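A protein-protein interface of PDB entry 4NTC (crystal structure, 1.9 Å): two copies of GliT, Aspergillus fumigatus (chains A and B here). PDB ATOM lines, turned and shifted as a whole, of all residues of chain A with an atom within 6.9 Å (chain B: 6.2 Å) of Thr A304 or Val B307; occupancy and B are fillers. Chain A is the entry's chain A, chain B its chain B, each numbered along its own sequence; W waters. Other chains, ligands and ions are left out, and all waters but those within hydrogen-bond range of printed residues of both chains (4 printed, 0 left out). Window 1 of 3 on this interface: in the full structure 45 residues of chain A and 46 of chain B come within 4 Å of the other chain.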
ATOM      1  N   PRO A  24     -29.037   6.013 -14.862  1.00  0.00           N
ATOM      2  CA  PRO A  24     -28.844   4.653 -15.367  1.00  0.00           C
ATOM      3  C   PRO A  24     -29.985   4.128 -16.249  1.00  0.00           C
ATOM      4  O   PRO A  24     -29.721   3.420 -17.226  1.00  0.00           O
ATOM      5  CB  PRO A  24     -28.738   3.818 -14.086  1.00  0.00           C
ATOM      6  CG  PRO A  24     -28.223   4.766 -13.067  1.00  0.00           C
ATOM      7  CD  PRO A  24     -28.843   6.088 -13.402  1.00  0.00           C
ATOM      8  N   HIS A  57     -23.265   0.849  -4.159  1.00  0.00           N
ATOM      9  CA  HIS A  57     -23.122  -0.548  -3.771  1.00  0.00           C
ATOM     10  C   HIS A  57     -24.215  -1.394  -4.393  1.00  0.00           C
ATOM     11  O   HIS A  57     -25.224  -0.865  -4.884  1.00  0.00           O
ATOM     12  CB  HIS A  57     -23.122  -0.695  -2.248  1.00  0.00           C
ATOM     13  CG  HIS A  57     -22.053   0.099  -1.570  1.00  0.00           C
ATOM     14  ND1 HIS A  57     -22.322   1.232  -0.833  1.00  0.00           N
ATOM     15  CD2 HIS A  57     -20.709  -0.062  -1.537  1.00  0.00           C
ATOM     16  CE1 HIS A  57     -21.191   1.727  -0.362  1.00  0.00           C
ATOM     17  NE2 HIS A  57     -20.199   0.960  -0.778  1.00  0.00           N
ATOM     18  N   ASN A  58     -23.998  -2.710  -4.386  1.00  0.00           N
ATOM     19  CA  ASN A  58     -24.961  -3.672  -4.904  1.00  0.00           C
ATOM     20  C   ASN A  58     -25.156  -3.540  -6.421  1.00  0.00           C
ATOM     21  O   ASN A  58     -26.209  -3.895  -6.957  1.00  0.00           O
ATOM     22  CB  ASN A  58     -26.300  -3.554  -4.157  1.00  0.00           C
ATOM     23  CG  ASN A  58     -27.085  -4.849  -4.158  1.00  0.00           C
ATOM     24  OD1 ASN A  58     -26.510  -5.935  -4.196  1.00  0.00           O
ATOM     25  ND2 ASN A  58     -28.405  -4.740  -4.121  1.00  0.00           N
ATOM     26  N   VAL A  59     -24.136  -3.016  -7.095  1.00  0.00           N
ATOM     27  CA  VAL A  59     -24.123  -2.921  -8.555  1.00  0.00           C
ATOM     28  C   VAL A  59     -22.913  -3.695  -9.082  1.00  0.00           C
ATOM     29  O   VAL A  59     -21.783  -3.209  -9.025  1.00  0.00           O
ATOM     30  CB  VAL A  59     -24.064  -1.452  -9.032  1.00  0.00           C
ATOM     31  CG1 VAL A  59     -24.226  -1.372 -10.546  1.00  0.00           C
ATOM     32  CG2 VAL A  59     -25.130  -0.617  -8.340  1.00  0.00           C
ATOM     33  N   LEU A  60     -23.162  -4.901  -9.590  1.00  0.00           N
ATOM     34  CA  LEU A  60     -22.096  -5.819 -10.010  1.00  0.00           C
ATOM     35  C   LEU A  60     -20.985  -5.157 -10.829  1.00  0.00           C
ATOM     36  O   LEU A  60     -21.235  -4.585 -11.898  1.00  0.00           O
ATOM     37  CB  LEU A  60     -22.671  -7.013 -10.778  1.00  0.00           C
ATOM     38  CG  LEU A  60     -21.649  -8.107 -11.101  1.00  0.00           C
ATOM     39  CD1 LEU A  60     -21.268  -8.877  -9.837  1.00  0.00           C
ATOM     40  CD2 LEU A  60     -22.188  -9.059 -12.155  1.00  0.00           C
ATOM     41  N   LEU A 300     -39.165  -1.011  -7.110  1.00  0.00           N
ATOM     42  CA  LEU A 300     -37.830  -1.609  -6.981  1.00  0.00           C
ATOM     43  C   LEU A 300     -36.784  -0.578  -7.384  1.00  0.00           C
ATOM     44  O   LEU A 300     -36.157  -0.682  -8.446  1.00  0.00           O
ATOM     45  CB  LEU A 300     -37.718  -2.865  -7.853  1.00  0.00           C
ATOM     46  CG  LEU A 300     -38.815  -3.930  -7.733  1.00  0.00           C
ATOM     47  CD1 LEU A 300     -38.724  -4.927  -8.885  1.00  0.00           C
ATOM     48  CD2 LEU A 300     -38.766  -4.644  -6.385  1.00  0.00           C
ATOM     49  N   ALA A 302     -33.647   0.763  -7.589  1.00  0.00           N
ATOM     50  CA  ALA A 302     -32.214   0.487  -7.498  1.00  0.00           C
ATOM     51  C   ALA A 302     -31.565   0.562  -8.872  1.00  0.00           C
ATOM     52  O   ALA A 302     -32.258   0.547  -9.897  1.00  0.00           O
ATOM     53  CB  ALA A 302     -31.969  -0.874  -6.857  1.00  0.00           C
ATOM     54  N   VAL A 303     -30.236   0.632  -8.886  1.00  0.00           N
ATOM     55  CA  VAL A 303     -29.490   0.767 -10.132  1.00  0.00           C
ATOM     56  C   VAL A 303     -29.651  -0.452 -11.057  1.00  0.00           C
ATOM     57  O   VAL A 303     -29.976  -0.276 -12.235  1.00  0.00           O
ATOM     58  CB  VAL A 303     -28.002   1.133  -9.890  1.00  0.00           C
ATOM     59  CG1 VAL A 303     -27.192   1.014 -11.176  1.00  0.00           C
ATOM     60  CG2 VAL A 303     -27.887   2.546  -9.326  1.00  0.00           C
ATOM     61  N   THR A 304     -29.454  -1.673 -10.552  1.00  0.00           N
ATOM     62  CA  THR A 304     -29.554  -2.850 -11.439  1.00  0.00           C
ATOM     63  C   THR A 304     -30.949  -3.079 -12.056  1.00  0.00           C
ATOM     64  O   THR A 304     -31.040  -3.414 -13.240  1.00  0.00           O
ATOM     65  CB  THR A 304     -28.951  -4.152 -10.843  1.00  0.00           C
ATOM     66  OG1 THR A 304     -29.734  -4.612  -9.735  1.00  0.00           O
ATOM     67  CG2 THR A 304     -27.503  -3.928 -10.410  1.00  0.00           C
ATOM     68  N   PRO A 305     -32.037  -2.900 -11.271  1.00  0.00           N
ATOM     69  CA  PRO A 305     -33.356  -2.944 -11.909  1.00  0.00           C
ATOM     70  C   PRO A 305     -33.586  -1.799 -12.905  1.00  0.00           C
ATOM     71  O   PRO A 305     -34.221  -2.017 -13.932  1.00  0.00           O
ATOM     72  CB  PRO A 305     -34.327  -2.823 -10.730  1.00  0.00           C
ATOM     73  CG  PRO A 305     -33.562  -3.329  -9.557  1.00  0.00           C
ATOM     74  CD  PRO A 305     -32.154  -2.876  -9.798  1.00  0.00           C
ATOM     75  N   ALA A 306     -33.086  -0.602 -12.606  1.00  0.00           N
ATOM     76  CA  ALA A 306     -33.219   0.539 -13.523  1.00  0.00           C
ATOM     77  C   ALA A 306     -32.586   0.278 -14.898  1.00  0.00           C
ATOM     78  O   ALA A 306     -33.162   0.635 -15.933  1.00  0.00           O
ATOM     79  CB  ALA A 306     -32.644   1.802 -12.896  1.00  0.00           C
ATOM     80  N   VAL A 307     -31.410  -0.346 -14.899  1.00  0.00           N
ATOM     81  CA  VAL A 307     -30.670  -0.657 -16.128  1.00  0.00           C
ATOM     82  C   VAL A 307     -31.360  -1.775 -16.910  1.00  0.00           C
ATOM     83  O   VAL A 307     -31.474  -1.711 -18.142  1.00  0.00           O
ATOM     84  CB  VAL A 307     -29.202  -1.034 -15.821  1.00  0.00           C
ATOM     85  CG1 VAL A 307     -28.503  -1.583 -17.060  1.00  0.00           C
ATOM     86  CG2 VAL A 307     -28.450   0.175 -15.292  1.00  0.00           C
ATOM     87  N   SER A 308     -31.828  -2.785 -16.182  1.00  0.00           N
ATOM     88  CA  SER A 308     -32.590  -3.880 -16.773  1.00  0.00           C
ATOM     89  C   SER A 308     -33.864  -3.362 -17.458  1.00  0.00           C
ATOM     90  O   SER A 308     -34.161  -3.740 -18.594  1.00  0.00           O
ATOM     91  CB  SER A 308     -32.938  -4.916 -15.701  1.00  0.00           C
ATOM     92  OG  SER A 308     -33.523  -6.062 -16.281  1.00  0.00           O
ATOM     93  N   MET A 309     -34.599  -2.486 -16.768  1.00  0.00           N
ATOM     94  CA  MET A 309     -35.815  -1.881 -17.324  1.00  0.00           C
ATOM     95  C   MET A 309     -35.496  -1.112 -18.601  1.00  0.00           C
ATOM     96  O   MET A 309     -36.245  -1.173 -19.576  1.00  0.00           O
ATOM     97  CB  MET A 309     -36.468  -0.934 -16.307  1.00  0.00           C
ATOM     98  CG  MET A 309     -37.190  -1.615 -15.157  1.00  0.00           C
ATOM     99  SD  MET A 309     -37.797  -0.374 -13.989  1.00  0.00           S
ATOM    100  CE  MET A 309     -39.359   0.065 -14.745  1.00  0.00           C
ATOM    101  N   PRO B  24     -22.687 -13.595 -14.345  1.00  0.00           N
ATOM    102  CA  PRO B  24     -23.263 -12.345 -13.857  1.00  0.00           C
ATOM    103  C   PRO B  24     -24.438 -12.559 -12.891  1.00  0.00           C
ATOM    104  O   PRO B  24     -24.569 -11.814 -11.917  1.00  0.00           O
ATOM    105  CB  PRO B  24     -23.741 -11.650 -15.139  1.00  0.00           C
ATOM    106  CG  PRO B  24     -22.895 -12.221 -16.220  1.00  0.00           C
ATOM    107  CD  PRO B  24     -22.593 -13.635 -15.815  1.00  0.00           C
ATOM    108  N   ALA B  25     -25.271 -13.568 -13.152  1.00  0.00           N
ATOM    109  CA  ALA B  25     -26.445 -13.837 -12.321  1.00  0.00           C
ATOM    110  C   ALA B  25     -26.075 -14.296 -10.909  1.00  0.00           C
ATOM    111  O   ALA B  25     -26.557 -13.727  -9.922  1.00  0.00           O
ATOM    112  CB  ALA B  25     -27.354 -14.857 -12.988  1.00  0.00           C
ATOM    113  N   SER B  28     -24.090 -11.460  -9.094  1.00  0.00           N
ATOM    114  CA  SER B  28     -25.012 -10.420  -8.641  1.00  0.00           C
ATOM    115  C   SER B  28     -25.772 -10.840  -7.379  1.00  0.00           C
ATOM    116  O   SER B  28     -25.973 -10.021  -6.473  1.00  0.00           O
ATOM    117  CB  SER B  28     -25.994 -10.015  -9.745  1.00  0.00           C
ATOM    118  OG  SER B  28     -26.807  -8.939  -9.306  1.00  0.00           O
ATOM    119  N   THR B  29     -26.190 -12.106  -7.323  1.00  0.00           N
ATOM    120  CA  THR B  29     -26.873 -12.647  -6.138  1.00  0.00           C
ATOM    121  C   THR B  29     -25.967 -12.572  -4.903  1.00  0.00           C
ATOM    122  O   THR B  29     -26.384 -12.075  -3.848  1.00  0.00           O
ATOM    123  CB  THR B  29     -27.344 -14.107  -6.340  1.00  0.00           C
ATOM    124  OG1 THR B  29     -28.053 -14.231  -7.578  1.00  0.00           O
ATOM    125  CG2 THR B  29     -28.262 -14.545  -5.199  1.00  0.00           C
ATOM    126  N   LEU B  70     -16.090  -8.543 -16.619  1.00  0.00           N
ATOM    127  CA  LEU B  70     -17.227  -8.367 -15.713  1.00  0.00           C
ATOM    128  C   LEU B  70     -17.196  -9.405 -14.589  1.00  0.00           C
ATOM    129  O   LEU B  70     -17.412  -9.068 -13.422  1.00  0.00           O
ATOM    130  CB  LEU B  70     -18.565  -8.423 -16.461  1.00  0.00           C
ATOM    131  CG  LEU B  70     -19.838  -8.350 -15.604  1.00  0.00           C
ATOM    132  CD1 LEU B  70     -19.938  -7.027 -14.848  1.00  0.00           C
ATOM    133  CD2 LEU B  70     -21.081  -8.577 -16.449  1.00  0.00           C
ATOM    134  N   GLY B 294     -30.831 -15.600 -13.881  1.00  0.00           N
ATOM    135  CA  GLY B 294     -30.056 -15.558 -15.113  1.00  0.00           C
ATOM    136  C   GLY B 294     -30.671 -16.423 -16.189  1.00  0.00           C
ATOM    137  O   GLY B 294     -31.862 -16.729 -16.141  1.00  0.00           O
ATOM    138  N   ALA B 302     -30.027 -12.118 -21.329  1.00  0.00           N
ATOM    139  CA  ALA B 302     -29.023 -11.070 -21.537  1.00  0.00           C
ATOM    140  C   ALA B 302     -28.396 -10.727 -20.193  1.00  0.00           C
ATOM    141  O   ALA B 302     -28.916 -11.123 -19.151  1.00  0.00           O
ATOM    142  CB  ALA B 302     -29.654  -9.836 -22.172  1.00  0.00           C
ATOM    143  N   VAL B 303     -27.292  -9.986 -20.212  1.00  0.00           N
ATOM    144  CA  VAL B 303     -26.533  -9.715 -18.986  1.00  0.00           C
ATOM    145  C   VAL B 303     -27.274  -8.802 -18.005  1.00  0.00           C
ATOM    146  O   VAL B 303     -27.342  -9.121 -16.821  1.00  0.00           O
ATOM    147  CB  VAL B 303     -25.114  -9.168 -19.286  1.00  0.00           C
ATOM    148  CG1 VAL B 303     -24.446  -8.648 -18.020  1.00  0.00           C
ATOM    149  CG2 VAL B 303     -24.251 -10.242 -19.936  1.00  0.00           C
ATOM    150  N   THR B 304     -27.837  -7.686 -18.477  1.00  0.00           N
ATOM    151  CA  THR B 304     -28.515  -6.769 -17.544  1.00  0.00           C
ATOM    152  C   THR B 304     -29.738  -7.381 -16.840  1.00  0.00           C
ATOM    153  O   THR B 304     -29.923  -7.138 -15.644  1.00  0.00           O
ATOM    154  CB  THR B 304     -28.839  -5.367 -18.136  1.00  0.00           C
ATOM    155  OG1 THR B 304     -29.878  -5.467 -19.118  1.00  0.00           O
ATOM    156  CG2 THR B 304     -27.596  -4.731 -18.753  1.00  0.00           C
ATOM    157  N   PRO B 305     -30.569  -8.181 -17.558  1.00  0.00           N
ATOM    158  CA  PRO B 305     -31.618  -8.885 -16.810  1.00  0.00           C
ATOM    159  C   PRO B 305     -31.070  -9.929 -15.837  1.00  0.00           C
ATOM    160  O   PRO B 305     -31.600 -10.063 -14.734  1.00  0.00           O
ATOM    161  CB  PRO B 305     -32.447  -9.567 -17.908  1.00  0.00           C
ATOM    162  CG  PRO B 305     -32.195  -8.756 -19.127  1.00  0.00           C
ATOM    163  CD  PRO B 305     -30.759  -8.339 -19.016  1.00  0.00           C
ATOM    164  N   ALA B 306     -30.022 -10.652 -16.235  1.00  0.00           N
ATOM    165  CA  ALA B 306     -29.383 -11.637 -15.355  1.00  0.00           C
ATOM    166  C   ALA B 306     -28.894 -10.987 -14.060  1.00  0.00           C
ATOM    167  O   ALA B 306     -29.035 -11.564 -12.977  1.00  0.00           O
ATOM    168  CB  ALA B 306     -28.229 -12.326 -16.069  1.00  0.00           C
ATOM    169  N   VAL B 307     -28.322  -9.790 -14.180  1.00  0.00           N
ATOM    170  CA  VAL B 307     -27.785  -9.062 -13.025  1.00  0.00           C
ATOM    171  C   VAL B 307     -28.919  -8.548 -12.128  1.00  0.00           C
ATOM    172  O   VAL B 307     -28.849  -8.668 -10.902  1.00  0.00           O
ATOM    173  CB  VAL B 307     -26.833  -7.917 -13.455  1.00  0.00           C
ATOM    174  CG1 VAL B 307     -26.468  -7.022 -12.277  1.00  0.00           C
ATOM    175  CG2 VAL B 307     -25.567  -8.470 -14.093  1.00  0.00           C
ATOM    176  N   SER B 308     -29.960  -7.988 -12.744  1.00  0.00           N
ATOM    177  CA  SER B 308     -31.133  -7.497 -12.011  1.00  0.00           C
ATOM    178  C   SER B 308     -31.842  -8.630 -11.268  1.00  0.00           C
ATOM    179  O   SER B 308     -32.281  -8.452 -10.131  1.00  0.00           O
ATOM    180  CB  SER B 308     -32.116  -6.810 -12.962  1.00  0.00           C
ATOM    181  OG  SER B 308     -33.225  -6.307 -12.244  1.00  0.00           O
ATOM    182  N   MET B 309     -31.953  -9.790 -11.920  1.00  0.00           N
ATOM    183  CA  MET B 309     -32.526 -10.973 -11.290  1.00  0.00           C
ATOM    184  C   MET B 309     -31.731 -11.373 -10.050  1.00  0.00           C
ATOM    185  O   MET B 309     -32.324 -11.688  -9.022  1.00  0.00           O
ATOM    186  CB  MET B 309     -32.582 -12.154 -12.261  1.00  0.00           C
ATOM    187  CG  MET B 309     -33.699 -12.086 -13.294  1.00  0.00           C
ATOM    188  SD  MET B 309     -33.606 -13.472 -14.445  1.00  0.00           S
ATOM    189  CE  MET B 309     -34.513 -14.744 -13.566  1.00  0.00           C
ATOM    190  N   GLY B 310     -30.402 -11.363 -10.161  1.00  0.00           N
ATOM    191  CA  GLY B 310     -29.514 -11.658  -9.036  1.00  0.00           C
ATOM    192  C   GLY B 310     -29.778 -10.756  -7.844  1.00  0.00           C
ATOM    193  O   GLY B 310     -29.861 -11.226  -6.706  1.00  0.00           O
ATOM    194  N   SER B 311     -29.933  -9.461  -8.107  1.00  0.00           N
ATOM    195  CA  SER B 311     -30.177  -8.479  -7.049  1.00  0.00           C
ATOM    196  C   SER B 311     -31.503  -8.707  -6.342  1.00  0.00           C
ATOM    197  O   SER B 311     -31.575  -8.645  -5.117  1.00  0.00           O
ATOM    198  CB  SER B 311     -30.157  -7.053  -7.609  1.00  0.00           C
ATOM    199  OG  SER B 311     -28.921  -6.756  -8.230  1.00  0.00           O
ATOM    200  N   LEU B 312     -32.551  -8.951  -7.123  1.00  0.00           N
ATOM    201  CA  LEU B 312     -33.886  -9.138  -6.572  1.00  0.00           C
ATOM    202  C   LEU B 312     -33.976 -10.483  -5.863  1.00  0.00           C
ATOM    203  O   LEU B 312     -34.574 -10.581  -4.789  1.00  0.00           O
ATOM    204  CB  LEU B 312     -34.948  -8.996  -7.667  1.00  0.00           C
ATOM    205  CG  LEU B 312     -35.064  -7.581  -8.256  1.00  0.00           C
ATOM    206  CD1 LEU B 312     -35.868  -7.597  -9.547  1.00  0.00           C
ATOM    207  CD2 LEU B 312     -35.657  -6.585  -7.261  1.00  0.00           C
HETATM  208  O   HOH W   1     -25.457  -6.230  -8.742  1.00  0.00           O
HETATM  209  O   HOH W   2     -30.067  -6.961  -3.402  1.00  0.00           O
HETATM  210  O   HOH W   3     -28.806  -4.780 -14.465  1.00  0.00           O
HETATM  211  O   HOH W   4     -27.004  -7.368  -6.423  1.00  0.00           O
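Among the printed residues, pairs that only touch across the chains: Leu A60 with Pro B24, Leu A60 with Ser B28, Leu A60 with Val B307, Leu A300 with Leu B312, Thr A304 with Val B307, Thr A304 with Ser B308, Pro A305 with Ser B308, Val A307 with Thr B304, Ser A308 with Thr B304, Ser A308 with Pro B305 and Ser A308 with Ser B308.
Thr A304 touches Val B307, and with the chains exchanged Val A307 touches Thr B304.
Thr A304 touches Ser B308, and with the chains exchanged Ser A308 touches Thr B304.
Pro A305 touches Ser B308, and with the chains exchanged Ser A308 touches Pro B305.
Ser B308 touches its own counterpart, Ser A308.
9 positions are printed for both chains.
Water W4 lies within hydrogen-bond range of OD1 of Asn A58 (2.7 Å), OG of Ser B311 (2.7 Å) and O of Ser B28 (2.8 Å).
Water W1 lies within hydrogen-bond range of the backbone NH (N) of Leu A60, the backbone carbonyl oxygen (O) of Asn A58 and the side-chain hydroxyl (OG) of Ser B28.
Water W2 bridges the backbone carbonyl oxygen of Ser B311 and the side-chain amide nitrogen of Asn A58.
Water W3 lies within hydrogen-bond range of the backbone carbonyl oxygen of Thr B304 (2.9 Å) and the backbone carbonyl oxygen of Thr A304 (2.9 Å).
Thr A304 touches three residues of chain B.
Of the printed residues of chain A, Val B307 touches Leu A60 (3.9 Å) and Thr A304 (3.8 Å).
Of the printed residues of chain B, Leu A300 touches Leu B312 (3.8 Å).
Of the printed residues of chain A, Ser B28 touches Leu A60.
Val A303 touches none of the printed residues of chain B.
Gly B294 touches none of the printed residues of chain A.
The nearest residue of chain B that does not touch Thr A304 is Thr B304 (4.6 Å).
The nearest residue of chain A that does not touch Val B307 is Val A59 (5.8 Å).
Of the 17 printed residues of chain B, 8 touch a printed residue of chain A.
Hydrophobic or aromatic side chains of chain B that line the printed part of chain A: Val B307 and Leu B312.
Of the 14 printed residues of chain A, 6 touch a printed residue of chain B.
Printed residues of chain A that touch a printed residue of chain B: Leu A60, Leu A300, Thr A304, Pro A305, Val A307 and Ser A308.
Hydrophobic or aromatic side chains of chain A that line the printed part of chain B: Leu A60, Leu A300, Pro A305 and Val A307.
Among the printed residues, 12 pairs touch across the chains.
The side-chain hydroxyl (OG) of Ser B311 sits at hydrogen-bond distance from the backbone carbonyl oxygen (O) of Val B307, at 3.3 Å.
OG of Ser B28 sits at hydrogen-bond distance from OG of Ser B311 (3.2 Å).
OG of Ser B28 is in hydrogen-bond range of O of Val B307, at 2.6 Å.
OG1 of Thr A304 lies within hydrogen-bond range of OG of Ser B311, 2.7 Å away.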
